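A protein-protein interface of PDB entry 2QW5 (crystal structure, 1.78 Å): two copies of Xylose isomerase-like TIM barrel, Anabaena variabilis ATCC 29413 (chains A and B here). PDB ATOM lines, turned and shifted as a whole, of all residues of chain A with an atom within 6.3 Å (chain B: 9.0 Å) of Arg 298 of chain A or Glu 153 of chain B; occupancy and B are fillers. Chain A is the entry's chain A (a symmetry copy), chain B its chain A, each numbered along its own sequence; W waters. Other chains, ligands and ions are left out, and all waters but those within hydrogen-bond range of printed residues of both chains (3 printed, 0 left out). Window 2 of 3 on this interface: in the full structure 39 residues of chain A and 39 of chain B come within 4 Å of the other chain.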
ATOM      1  N   ASN A 284     -39.205  24.941  -0.857  1.00  0.00           N
ATOM      2  CA  ASN A 284     -38.840  24.985   0.566  1.00  0.00           C
ATOM      3  C   ASN A 284     -37.465  24.305   0.784  1.00  0.00           C
ATOM      4  O   ASN A 284     -37.023  23.502  -0.036  1.00  0.00           O
ATOM      5  CB  ASN A 284     -39.972  24.372   1.391  1.00  0.00           C
ATOM      6  CG  ASN A 284     -39.885  24.709   2.853  1.00  0.00           C
ATOM      7  OD1 ASN A 284     -39.059  25.533   3.248  1.00  0.00           O
ATOM      8  ND2 ASN A 284     -40.753  24.076   3.684  1.00  0.00           N
ATOM      9  N   ALA A 285     -36.751  24.672   1.843  1.00  0.00           N
ATOM     10  CA  ALA A 285     -35.463  24.020   2.179  1.00  0.00           C
ATOM     11  C   ALA A 285     -35.734  22.617   2.787  1.00  0.00           C
ATOM     12  O   ALA A 285     -35.587  22.381   3.981  1.00  0.00           O
ATOM     13  CB  ALA A 285     -34.601  24.916   3.082  1.00  0.00           C
ATOM     14  N   LEU A 295     -29.211  25.725  -0.827  1.00  0.00           N
ATOM     15  CA  LEU A 295     -30.059  26.517   0.019  1.00  0.00           C
ATOM     16  C   LEU A 295     -29.416  26.760   1.376  1.00  0.00           C
ATOM     17  O   LEU A 295     -29.372  25.883   2.209  1.00  0.00           O
ATOM     18  CB  LEU A 295     -31.454  25.875   0.168  1.00  0.00           C
ATOM     19  CG  LEU A 295     -32.291  25.713  -1.114  1.00  0.00           C
ATOM     20  CD1 LEU A 295     -33.609  24.967  -0.817  1.00  0.00           C
ATOM     21  CD2 LEU A 295     -32.502  27.074  -1.779  1.00  0.00           C
ATOM     22  N   THR A 296     -28.907  27.970   1.547  1.00  0.00           N
ATOM     23  CA  THR A 296     -28.279  28.407   2.778  1.00  0.00           C
ATOM     24  C   THR A 296     -29.350  28.998   3.728  1.00  0.00           C
ATOM     25  O   THR A 296     -29.112  29.109   4.932  1.00  0.00           O
ATOM     26  CB  THR A 296     -27.185  29.439   2.509  1.00  0.00           C
ATOM     27  OG1 THR A 296     -27.804  30.624   2.023  1.00  0.00           O
ATOM     28  CG2 THR A 296     -26.112  28.917   1.447  1.00  0.00           C
ATOM     29  N   ARG A 297     -30.517  29.378   3.186  1.00  0.00           N
ATOM     30  CA  ARG A 297     -31.605  29.943   3.977  1.00  0.00           C
ATOM     31  C   ARG A 297     -32.282  28.913   4.877  1.00  0.00           C
ATOM     32  O   ARG A 297     -32.370  27.722   4.547  1.00  0.00           O
ATOM     33  CB  ARG A 297     -32.676  30.598   3.088  1.00  0.00           C
ATOM     34  CG  ARG A 297     -33.326  29.703   1.968  1.00  0.00           C
ATOM     35  CD  ARG A 297     -34.453  30.446   1.257  1.00  0.00           C
ATOM     36  NE  ARG A 297     -34.685  29.944  -0.103  1.00  0.00           N
ATOM     37  CZ  ARG A 297     -35.453  28.913  -0.451  1.00  0.00           C
ATOM     38  NH1 ARG A 297     -36.100  28.203   0.453  1.00  0.00           N
ATOM     39  NH2 ARG A 297     -35.549  28.584  -1.744  1.00  0.00           N
ATOM     40  N   ARG A 298     -32.852  29.410   5.964  1.00  0.00           N
ATOM     41  CA  ARG A 298     -33.584  28.536   6.864  1.00  0.00           C
ATOM     42  C   ARG A 298     -34.888  28.012   6.218  1.00  0.00           C
ATOM     43  O   ARG A 298     -35.505  28.676   5.348  1.00  0.00           O
ATOM     44  CB  ARG A 298     -33.931  29.251   8.167  1.00  0.00           C
ATOM     45  CG  ARG A 298     -32.754  29.616   8.992  1.00  0.00           C
ATOM     46  CD  ARG A 298     -33.227  30.175  10.331  1.00  0.00           C
ATOM     47  NE  ARG A 298     -32.090  30.604  11.138  1.00  0.00           N
ATOM     48  CZ  ARG A 298     -31.334  29.819  11.918  1.00  0.00           C
ATOM     49  NH1 ARG A 298     -31.552  28.506  12.052  1.00  0.00           N
ATOM     50  NH2 ARG A 298     -30.314  30.364  12.580  1.00  0.00           N
ATOM     51  N   LYS A 299     -35.269  26.817   6.668  1.00  0.00           N
ATOM     52  CA  LYS A 299     -36.470  26.137   6.221  1.00  0.00           C
ATOM     53  C   LYS A 299     -37.710  26.879   6.733  1.00  0.00           C
ATOM     54  O   LYS A 299     -37.717  27.402   7.846  1.00  0.00           O
ATOM     55  CB  LYS A 299     -36.493  24.688   6.749  1.00  0.00           C
ATOM     56  CG  LYS A 299     -37.679  23.819   6.264  1.00  0.00           C
ATOM     57  CD  LYS A 299     -37.586  22.402   6.788  1.00  0.00           C
ATOM     58  CE  LYS A 299     -38.603  21.485   6.136  1.00  0.00           C
ATOM     59  NZ  LYS A 299     -38.586  20.111   6.747  1.00  0.00           N
ATOM     60  N   PHE A 300     -38.743  26.929   5.887  1.00  0.00           N
ATOM     61  CA  PHE A 300     -40.069  27.418   6.308  1.00  0.00           C
ATOM     62  C   PHE A 300     -40.691  26.141   6.874  1.00  0.00           C
ATOM     63  O   PHE A 300     -41.206  25.285   6.130  1.00  0.00           O
ATOM     64  CB  PHE A 300     -40.893  27.989   5.158  1.00  0.00           C
ATOM     65  CG  PHE A 300     -40.126  28.908   4.263  1.00  0.00           C
ATOM     66  CD1 PHE A 300     -39.440  29.993   4.792  1.00  0.00           C
ATOM     67  CD2 PHE A 300     -40.133  28.724   2.877  1.00  0.00           C
ATOM     68  CE1 PHE A 300     -38.761  30.886   3.983  1.00  0.00           C
ATOM     69  CE2 PHE A 300     -39.453  29.621   2.048  1.00  0.00           C
ATOM     70  CZ  PHE A 300     -38.743  30.693   2.608  1.00  0.00           C
ATOM     71  N   ASN A 309     -40.698  26.667  15.448  1.00  0.00           N
ATOM     72  CA  ASN A 309     -39.602  27.517  15.866  1.00  0.00           C
ATOM     73  C   ASN A 309     -40.027  28.956  15.667  1.00  0.00           C
ATOM     74  O   ASN A 309     -41.126  29.213  15.162  1.00  0.00           O
ATOM     75  CB  ASN A 309     -38.271  27.139  15.165  1.00  0.00           C
ATOM     76  CG  ASN A 309     -38.245  27.451  13.654  1.00  0.00           C
ATOM     77  OD1 ASN A 309     -38.717  28.490  13.208  1.00  0.00           O
ATOM     78  ND2 ASN A 309     -37.618  26.578  12.889  1.00  0.00           N
ATOM     79  N   TYR A 311     -39.095  31.148  13.497  1.00  0.00           N
ATOM     80  CA  TYR A 311     -39.018  31.636  12.114  1.00  0.00           C
ATOM     81  C   TYR A 311     -40.351  31.411  11.388  1.00  0.00           C
ATOM     82  O   TYR A 311     -41.229  30.730  11.925  1.00  0.00           O
ATOM     83  CB  TYR A 311     -37.830  30.981  11.403  1.00  0.00           C
ATOM     84  CG  TYR A 311     -36.542  31.221  12.163  1.00  0.00           C
ATOM     85  CD1 TYR A 311     -35.983  32.486  12.214  1.00  0.00           C
ATOM     86  CD2 TYR A 311     -35.898  30.186  12.855  1.00  0.00           C
ATOM     87  CE1 TYR A 311     -34.786  32.723  12.942  1.00  0.00           C
ATOM     88  CE2 TYR A 311     -34.717  30.404  13.572  1.00  0.00           C
ATOM     89  CZ  TYR A 311     -34.169  31.679  13.610  1.00  0.00           C
ATOM     90  OH  TYR A 311     -33.003  31.910  14.305  1.00  0.00           O
ATOM     91  N   ILE B 146     -23.673  20.562   4.583  1.00  0.00           N
ATOM     92  CA  ILE B 146     -24.320  21.298   5.674  1.00  0.00           C
ATOM     93  C   ILE B 146     -25.027  22.514   5.047  1.00  0.00           C
ATOM     94  O   ILE B 146     -24.373  23.435   4.511  1.00  0.00           O
ATOM     95  CB  ILE B 146     -23.334  21.757   6.774  1.00  0.00           C
ATOM     96  CG1 ILE B 146     -22.593  20.550   7.389  1.00  0.00           C
ATOM     97  CG2 ILE B 146     -24.084  22.523   7.872  1.00  0.00           C
ATOM     98  CD1 ILE B 146     -21.317  20.901   8.171  1.00  0.00           C
ATOM     99  N   TRP B 147     -26.356  22.516   5.156  1.00  0.00           N
ATOM    100  CA  TRP B 147     -27.207  23.567   4.591  1.00  0.00           C
ATOM    101  C   TRP B 147     -28.238  24.125   5.572  1.00  0.00           C
ATOM    102  O   TRP B 147     -28.367  23.635   6.702  1.00  0.00           O
ATOM    103  CB  TRP B 147     -27.953  22.965   3.378  1.00  0.00           C
ATOM    104  CG  TRP B 147     -27.108  22.514   2.251  1.00  0.00           C
ATOM    105  CD1 TRP B 147     -26.906  21.227   1.847  1.00  0.00           C
ATOM    106  CD2 TRP B 147     -26.358  23.333   1.367  1.00  0.00           C
ATOM    107  NE1 TRP B 147     -26.057  21.201   0.758  1.00  0.00           N
ATOM    108  CE2 TRP B 147     -25.727  22.483   0.435  1.00  0.00           C
ATOM    109  CE3 TRP B 147     -26.170  24.707   1.255  1.00  0.00           C
ATOM    110  CZ2 TRP B 147     -24.894  22.977  -0.581  1.00  0.00           C
ATOM    111  CZ3 TRP B 147     -25.384  25.192   0.245  1.00  0.00           C
ATOM    112  CH2 TRP B 147     -24.734  24.323  -0.651  1.00  0.00           C
ATOM    113  N   SER B 148     -28.954  25.148   5.096  1.00  0.00           N
ATOM    114  CA  SER B 148     -30.118  25.745   5.725  1.00  0.00           C
ATOM    115  C   SER B 148     -29.912  26.012   7.218  1.00  0.00           C
ATOM    116  O   SER B 148     -28.884  26.593   7.596  1.00  0.00           O
ATOM    117  CB  SER B 148     -31.385  24.898   5.384  1.00  0.00           C
ATOM    118  OG  SER B 148     -32.585  25.466   5.931  1.00  0.00           O
ATOM    119  N   ASP B 149     -30.830  25.577   8.072  1.00  0.00           N
ATOM    120  CA  ASP B 149     -30.745  25.926   9.484  1.00  0.00           C
ATOM    121  C   ASP B 149     -29.446  25.535  10.122  1.00  0.00           C
ATOM    122  O   ASP B 149     -28.846  26.358  10.821  1.00  0.00           O
ATOM    123  CB  ASP B 149     -31.928  25.372  10.280  1.00  0.00           C
ATOM    124  CG  ASP B 149     -33.254  25.910   9.782  1.00  0.00           C
ATOM    125  OD1 ASP B 149     -33.600  25.650   8.606  1.00  0.00           O
ATOM    126  OD2 ASP B 149     -33.954  26.589  10.555  1.00  0.00           O
ATOM    127  N   GLU B 150     -29.005  24.316   9.836  1.00  0.00           N
ATOM    128  CA  GLU B 150     -27.737  23.799  10.359  1.00  0.00           C
ATOM    129  C   GLU B 150     -26.550  24.670   9.883  1.00  0.00           C
ATOM    130  O   GLU B 150     -25.675  25.021  10.663  1.00  0.00           O
ATOM    131  CB  GLU B 150     -27.550  22.340   9.937  1.00  0.00           C
ATOM    132  CG  GLU B 150     -26.424  21.640  10.681  1.00  0.00           C
ATOM    133  CD  GLU B 150     -26.161  20.231  10.214  1.00  0.00           C
ATOM    134  OE1 GLU B 150     -26.699  19.792   9.159  1.00  0.00           O
ATOM    135  OE2 GLU B 150     -25.356  19.568  10.913  1.00  0.00           O
ATOM    136  N   LEU B 151     -26.532  25.027   8.616  1.00  0.00           N
ATOM    137  CA  LEU B 151     -25.498  25.914   8.093  1.00  0.00           C
ATOM    138  C   LEU B 151     -25.502  27.276   8.804  1.00  0.00           C
ATOM    139  O   LEU B 151     -24.437  27.789   9.161  1.00  0.00           O
ATOM    140  CB  LEU B 151     -25.633  26.138   6.560  1.00  0.00           C
ATOM    141  CG  LEU B 151     -24.627  27.091   5.954  1.00  0.00           C
ATOM    142  CD1 LEU B 151     -23.179  26.621   6.232  1.00  0.00           C
ATOM    143  CD2 LEU B 151     -24.907  27.211   4.433  1.00  0.00           C
ATOM    144  N   GLN B 152     -26.686  27.841   9.025  1.00  0.00           N
ATOM    145  CA  GLN B 152     -26.802  29.165   9.693  1.00  0.00           C
ATOM    146  C   GLN B 152     -26.273  29.116  11.144  1.00  0.00           C
ATOM    147  O   GLN B 152     -25.618  30.044  11.569  1.00  0.00           O
ATOM    148  CB  GLN B 152     -28.238  29.740   9.590  1.00  0.00           C
ATOM    149  CG  GLN B 152     -28.636  30.124   8.130  1.00  0.00           C
ATOM    150  CD  GLN B 152     -27.724  31.172   7.501  1.00  0.00           C
ATOM    151  OE1 GLN B 152     -27.262  32.078   8.188  1.00  0.00           O
ATOM    152  NE2 GLN B 152     -27.442  31.050   6.178  1.00  0.00           N
ATOM    153  N   GLU B 153     -26.510  28.022  11.855  1.00  0.00           N
ATOM    154  CA  GLU B 153     -25.967  27.834  13.214  1.00  0.00           C
ATOM    155  C   GLU B 153     -24.438  27.742  13.189  1.00  0.00           C
ATOM    156  O   GLU B 153     -23.775  28.379  14.018  1.00  0.00           O
ATOM    157  CB  GLU B 153     -26.587  26.610  13.915  1.00  0.00           C
ATOM    158  CG  GLU B 153     -28.048  26.763  14.232  1.00  0.00           C
ATOM    159  CD  GLU B 153     -28.316  27.957  15.178  1.00  0.00           C
ATOM    160  OE1 GLU B 153     -27.640  28.106  16.229  1.00  0.00           O
ATOM    161  OE2 GLU B 153     -29.183  28.771  14.843  1.00  0.00           O
ATOM    162  N   HIS B 154     -23.909  26.980  12.213  1.00  0.00           N
ATOM    163  CA  HIS B 154     -22.467  26.832  11.953  1.00  0.00           C
ATOM    164  C   HIS B 154     -21.822  28.189  11.652  1.00  0.00           C
ATOM    165  O   HIS B 154     -20.733  28.529  12.170  1.00  0.00           O
ATOM    166  CB  HIS B 154     -22.249  25.884  10.749  1.00  0.00           C
ATOM    167  CG  HIS B 154     -20.825  25.756  10.294  1.00  0.00           C
ATOM    168  ND1 HIS B 154     -20.015  24.709  10.674  1.00  0.00           N
ATOM    169  CD2 HIS B 154     -20.080  26.518   9.460  1.00  0.00           C
ATOM    170  CE1 HIS B 154     -18.823  24.856  10.127  1.00  0.00           C
ATOM    171  NE2 HIS B 154     -18.838  25.946   9.395  1.00  0.00           N
ATOM    172  N   LEU B 155     -22.471  28.963  10.772  1.00  0.00           N
ATOM    173  CA  LEU B 155     -21.953  30.277  10.391  1.00  0.00           C
ATOM    174  C   LEU B 155     -21.856  31.296  11.517  1.00  0.00           C
ATOM    175  O   LEU B 155     -21.019  32.190  11.435  1.00  0.00           O
ATOM    176  CB  LEU B 155     -22.698  30.870   9.203  1.00  0.00           C
ATOM    177  CG  LEU B 155     -22.511  30.214   7.833  1.00  0.00           C
ATOM    178  CD1 LEU B 155     -23.547  30.780   6.861  1.00  0.00           C
ATOM    179  CD2 LEU B 155     -21.073  30.354   7.293  1.00  0.00           C
ATOM    180  N   LYS B 156     -22.694  31.179  12.555  1.00  0.00           N
ATOM    181  CA  LYS B 156     -22.596  32.104  13.713  1.00  0.00           C
ATOM    182  C   LYS B 156     -21.240  32.004  14.386  1.00  0.00           C
ATOM    183  O   LYS B 156     -20.671  33.027  14.777  1.00  0.00           O
ATOM    184  CB  LYS B 156     -23.675  31.832  14.760  1.00  0.00           C
ATOM    185  CG  LYS B 156     -25.102  32.074  14.315  1.00  0.00           C
ATOM    186  CD  LYS B 156     -26.055  31.576  15.430  1.00  0.00           C
ATOM    187  CE  LYS B 156     -27.507  31.772  15.029  1.00  0.00           C
ATOM    188  NZ  LYS B 156     -28.422  31.388  16.132  1.00  0.00           N
ATOM    189  N   VAL B 157     -20.715  30.777  14.481  1.00  0.00           N
ATOM    190  CA  VAL B 157     -19.411  30.529  15.112  1.00  0.00           C
ATOM    191  C   VAL B 157     -18.290  31.081  14.215  1.00  0.00           C
ATOM    192  O   VAL B 157     -17.371  31.720  14.710  1.00  0.00           O
ATOM    193  CB  VAL B 157     -19.178  29.035  15.435  1.00  0.00           C
ATOM    194  CG1 VAL B 157     -17.807  28.819  16.130  1.00  0.00           C
ATOM    195  CG2 VAL B 157     -20.305  28.485  16.262  1.00  0.00           C
ATOM    196  N   ARG B 158     -18.413  30.878  12.896  1.00  0.00           N
ATOM    197  CA  ARG B 158     -17.430  31.362  11.930  1.00  0.00           C
ATOM    198  C   ARG B 158     -17.387  32.883  11.927  1.00  0.00           C
ATOM    199  O   ARG B 158     -16.297  33.480  11.991  1.00  0.00           O
ATOM    200  CB  ARG B 158     -17.757  30.846  10.515  1.00  0.00           C
ATOM    201  CG  ARG B 158     -17.826  29.309  10.393  1.00  0.00           C
ATOM    202  CD  ARG B 158     -16.460  28.612  10.466  1.00  0.00           C
ATOM    203  NE  ARG B 158     -15.698  28.924   9.252  1.00  0.00           N
ATOM    204  CZ  ARG B 158     -15.829  28.325   8.065  1.00  0.00           C
ATOM    205  NH1 ARG B 158     -16.654  27.296   7.882  1.00  0.00           N
ATOM    206  NH2 ARG B 158     -15.099  28.755   7.040  1.00  0.00           N
ATOM    207  N   TYR B 159     -18.559  33.520  11.917  1.00  0.00           N
ATOM    208  CA  TYR B 159     -18.622  34.985  11.971  1.00  0.00           C
ATOM    209  C   TYR B 159     -18.010  35.529  13.281  1.00  0.00           C
ATOM    210  O   TYR B 159     -17.247  36.475  13.237  1.00  0.00           O
ATOM    211  CB  TYR B 159     -20.044  35.505  11.747  1.00  0.00           C
ATOM    212  CG  TYR B 159     -20.600  35.243  10.349  1.00  0.00           C
ATOM    213  CD1 TYR B 159     -19.826  35.441   9.199  1.00  0.00           C
ATOM    214  CD2 TYR B 159     -21.927  34.871  10.177  1.00  0.00           C
ATOM    215  CE1 TYR B 159     -20.366  35.196   7.906  1.00  0.00           C
ATOM    216  CE2 TYR B 159     -22.478  34.621   8.897  1.00  0.00           C
ATOM    217  CZ  TYR B 159     -21.698  34.803   7.771  1.00  0.00           C
ATOM    218  OH  TYR B 159     -22.268  34.566   6.544  1.00  0.00           O
ATOM    219  N   ALA B 160     -18.313  34.904  14.428  1.00  0.00           N
ATOM    220  CA  ALA B 160     -17.697  35.297  15.729  1.00  0.00           C
ATOM    221  C   ALA B 160     -16.159  35.168  15.718  1.00  0.00           C
ATOM    222  O   ALA B 160     -15.447  36.064  16.220  1.00  0.00           O
ATOM    223  CB  ALA B 160     -18.296  34.523  16.881  1.00  0.00           C
ATOM    224  N   ASN B 194     -24.407  35.793   2.243  1.00  0.00           N
ATOM    225  CA  ASN B 194     -25.119  35.841   0.964  1.00  0.00           C
ATOM    226  C   ASN B 194     -25.902  37.132   0.718  1.00  0.00           C
ATOM    227  O   ASN B 194     -25.985  37.611  -0.434  1.00  0.00           O
ATOM    228  CB  ASN B 194     -26.071  34.640   0.782  1.00  0.00           C
ATOM    229  CG  ASN B 194     -25.386  33.290   0.944  1.00  0.00           C
ATOM    230  OD1 ASN B 194     -25.849  32.458   1.732  1.00  0.00           O
ATOM    231  ND2 ASN B 194     -24.271  33.087   0.254  1.00  0.00           N
ATOM    232  N   LYS B 195     -26.476  37.673   1.802  1.00  0.00           N
ATOM    233  CA  LYS B 195     -27.304  38.870   1.785  1.00  0.00           C
ATOM    234  C   LYS B 195     -26.663  40.043   2.510  1.00  0.00           C
ATOM    235  O   LYS B 195     -25.853  39.874   3.425  1.00  0.00           O
ATOM    236  CB  LYS B 195     -28.635  38.584   2.478  1.00  0.00           C
ATOM    237  CG  LYS B 195     -29.395  37.451   1.915  1.00  0.00           C
ATOM    238  CD  LYS B 195     -30.459  36.937   2.870  1.00  0.00           C
ATOM    239  CE  LYS B 195     -31.678  37.792   2.884  1.00  0.00           C
ATOM    240  NZ  LYS B 195     -32.756  37.025   3.575  1.00  0.00           N
ATOM    241  N   GLN B 198     -27.108  39.883   6.224  1.00  0.00           N
ATOM    242  CA  GLN B 198     -26.136  39.005   6.890  1.00  0.00           C
ATOM    243  C   GLN B 198     -24.787  39.716   7.066  1.00  0.00           C
ATOM    244  O   GLN B 198     -24.129  39.542   8.087  1.00  0.00           O
ATOM    245  CB  GLN B 198     -25.956  37.694   6.089  1.00  0.00           C
ATOM    246  CG  GLN B 198     -27.248  36.845   6.043  1.00  0.00           C
ATOM    247  CD  GLN B 198     -27.260  35.747   5.017  1.00  0.00           C
ATOM    248  OE1 GLN B 198     -26.516  35.800   4.021  1.00  0.00           O
ATOM    249  NE2 GLN B 198     -28.087  34.709   5.265  1.00  0.00           N
ATOM    250  N   GLU B 201     -25.189  42.462   9.760  1.00  0.00           N
ATOM    251  CA  GLU B 201     -25.111  41.793  11.077  1.00  0.00           C
ATOM    252  C   GLU B 201     -23.655  41.461  11.499  1.00  0.00           C
ATOM    253  O   GLU B 201     -23.274  41.662  12.655  1.00  0.00           O
ATOM    254  CB  GLU B 201     -25.974  40.533  11.065  1.00  0.00           C
ATOM    255  CG  GLU B 201     -26.103  39.809  12.440  1.00  0.00           C
ATOM    256  CD  GLU B 201     -27.154  38.660  12.453  1.00  0.00           C
ATOM    257  OE1 GLU B 201     -27.895  38.437  11.442  1.00  0.00           O
ATOM    258  OE2 GLU B 201     -27.229  37.978  13.503  1.00  0.00           O
HETATM  259  O   HOH W   1     -32.103  29.202  15.842  1.00  0.00           O
HETATM  260  O   HOH W   2     -29.091  33.006   3.069  1.00  0.00           O
HETATM  261  O   HOH W   3     -36.574  26.545  10.225  1.00  0.00           O
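The guanidinium group of Arg 298 of chain A lies within salt-bridge range of the side-chain carboxylate of Glu 153 of chain B, at 3.0 Å.
The side-chain carboxylate (OD2) of Asp 149 of chain B is in salt-bridge range of the guanidinium group (NH1) of Arg 298 of chain A.
OD1 of Asp 149 of chain B lies within hydrogen-bond range of N of Lys 299 of chain A, 2.8 Å away.
O of Thr 296 of chain A sits at hydrogen-bond distance from NE2 of Gln 152 of chain B (2.8 Å).
The backbone carbonyl oxygen (O) of Arg 297 of chain A lies within hydrogen-bond range of the side-chain hydroxyl (OG) of Ser 148 of chain B (2.7 Å).
OG of Ser 148 of chain B is in hydrogen-bond range of N of Lys 299 of chain A, at 3.1 Å.
N of Ser 148 of chain B is in hydrogen-bond range of O of Leu 295 of chain A (3.0 Å).
The side-chain hydroxyl (OG1) of Thr 296 of chain A lies within hydrogen-bond range of the side-chain amide oxygen (OD1) of Asn 194 of chain B.
Water W3 lies within hydrogen-bond range of the side-chain carboxylate (OD2) of Asp 149 of chain B (2.6 Å), the backbone carbonyl oxygen (O) of Lys 299 of chain A (2.8 Å) and the side-chain amide nitrogen (ND2) of Asn 309 of chain A (2.9 Å).
Water W2 lies within hydrogen-bond range of OG1 of Thr 296 of chain A (2.9 Å) and NE2 of Gln 198 of chain B (3.0 Å).
Water W1 bridges the side-chain carboxylate (OE2) of Glu 153 of chain B (3.1 Å) and the side-chain hydroxyl (OH) of Tyr 311 of chain A (3.2 Å).
Of the 19 printed residues of chain B, 8 touch a printed residue of chain A.
Printed residues of chain B that touch a printed residue of chain A: Trp 147, Ser 148, Asp 149, Leu 151, Gln 152, Glu 153, Lys 156 and Asn 194.
Of the 10 printed residues of chain A, 6 touch a printed residue of chain B.
Among the printed residues, merely in contact across the chains: Arg 298 of chain A with Ser 148 of chain B, Leu 295 of chain A with Trp 147 of chain B, Ala 285 of chain A with Ser 148 of chain B, Thr 296 of chain A with Ser 148 of chain B, Thr 296 of chain A with Leu 151 of chain B, Arg 298 of chain A with Gln 152 of chain B, Thr 296 of chain A with Trp 147 of chain B and Arg 298 of chain A with Lys 156 of chain B.
No position is printed for both chains.
Of the 16 pairs that touch across the chains among the printed residues, none has its exchanged pair printed and touching as well.
The side-chain carboxylate of Asp 149 of chain B sits at hydrogen-bond distance from the side-chain hydroxyl of Ser 148 of chain B, 2.9 Å away.
The side-chain amino group of Lys 156 of chain B lies within salt-bridge range of the side-chain carboxylate of Glu 153 of chain B, 3.0 Å away.
N of Asn 194 of chain B lies within hydrogen-bond range of OE1 of Gln 198 of chain B, 2.8 Å away.
Of the printed residues of chain B, Arg 298 of chain A touches Ser 148, Asp 149, Gln 152, Glu 153 and Lys 156.
Glu 153 of chain B touches one residue of chain A.
Printed residues of chain A within 4 Å of Trp 147 of chain B: Leu 295 (3.4 Å) and Thr 296 (3.98 Å).
Printed residues of chain B within 4 Å of Arg 297 of chain A: Ser 148 (2.7 Å).
Of the printed residues of chain A, Leu 151 of chain B touches Thr 296 (3.6 Å).
The nearest residue of chain A that does not touch Glu 153 of chain B is Tyr 311 of chain A (5.0 Å).
The nearest printed residue of chain B that does not touch Thr 296 of chain A is Asp 149 of chain B (5.0 Å).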
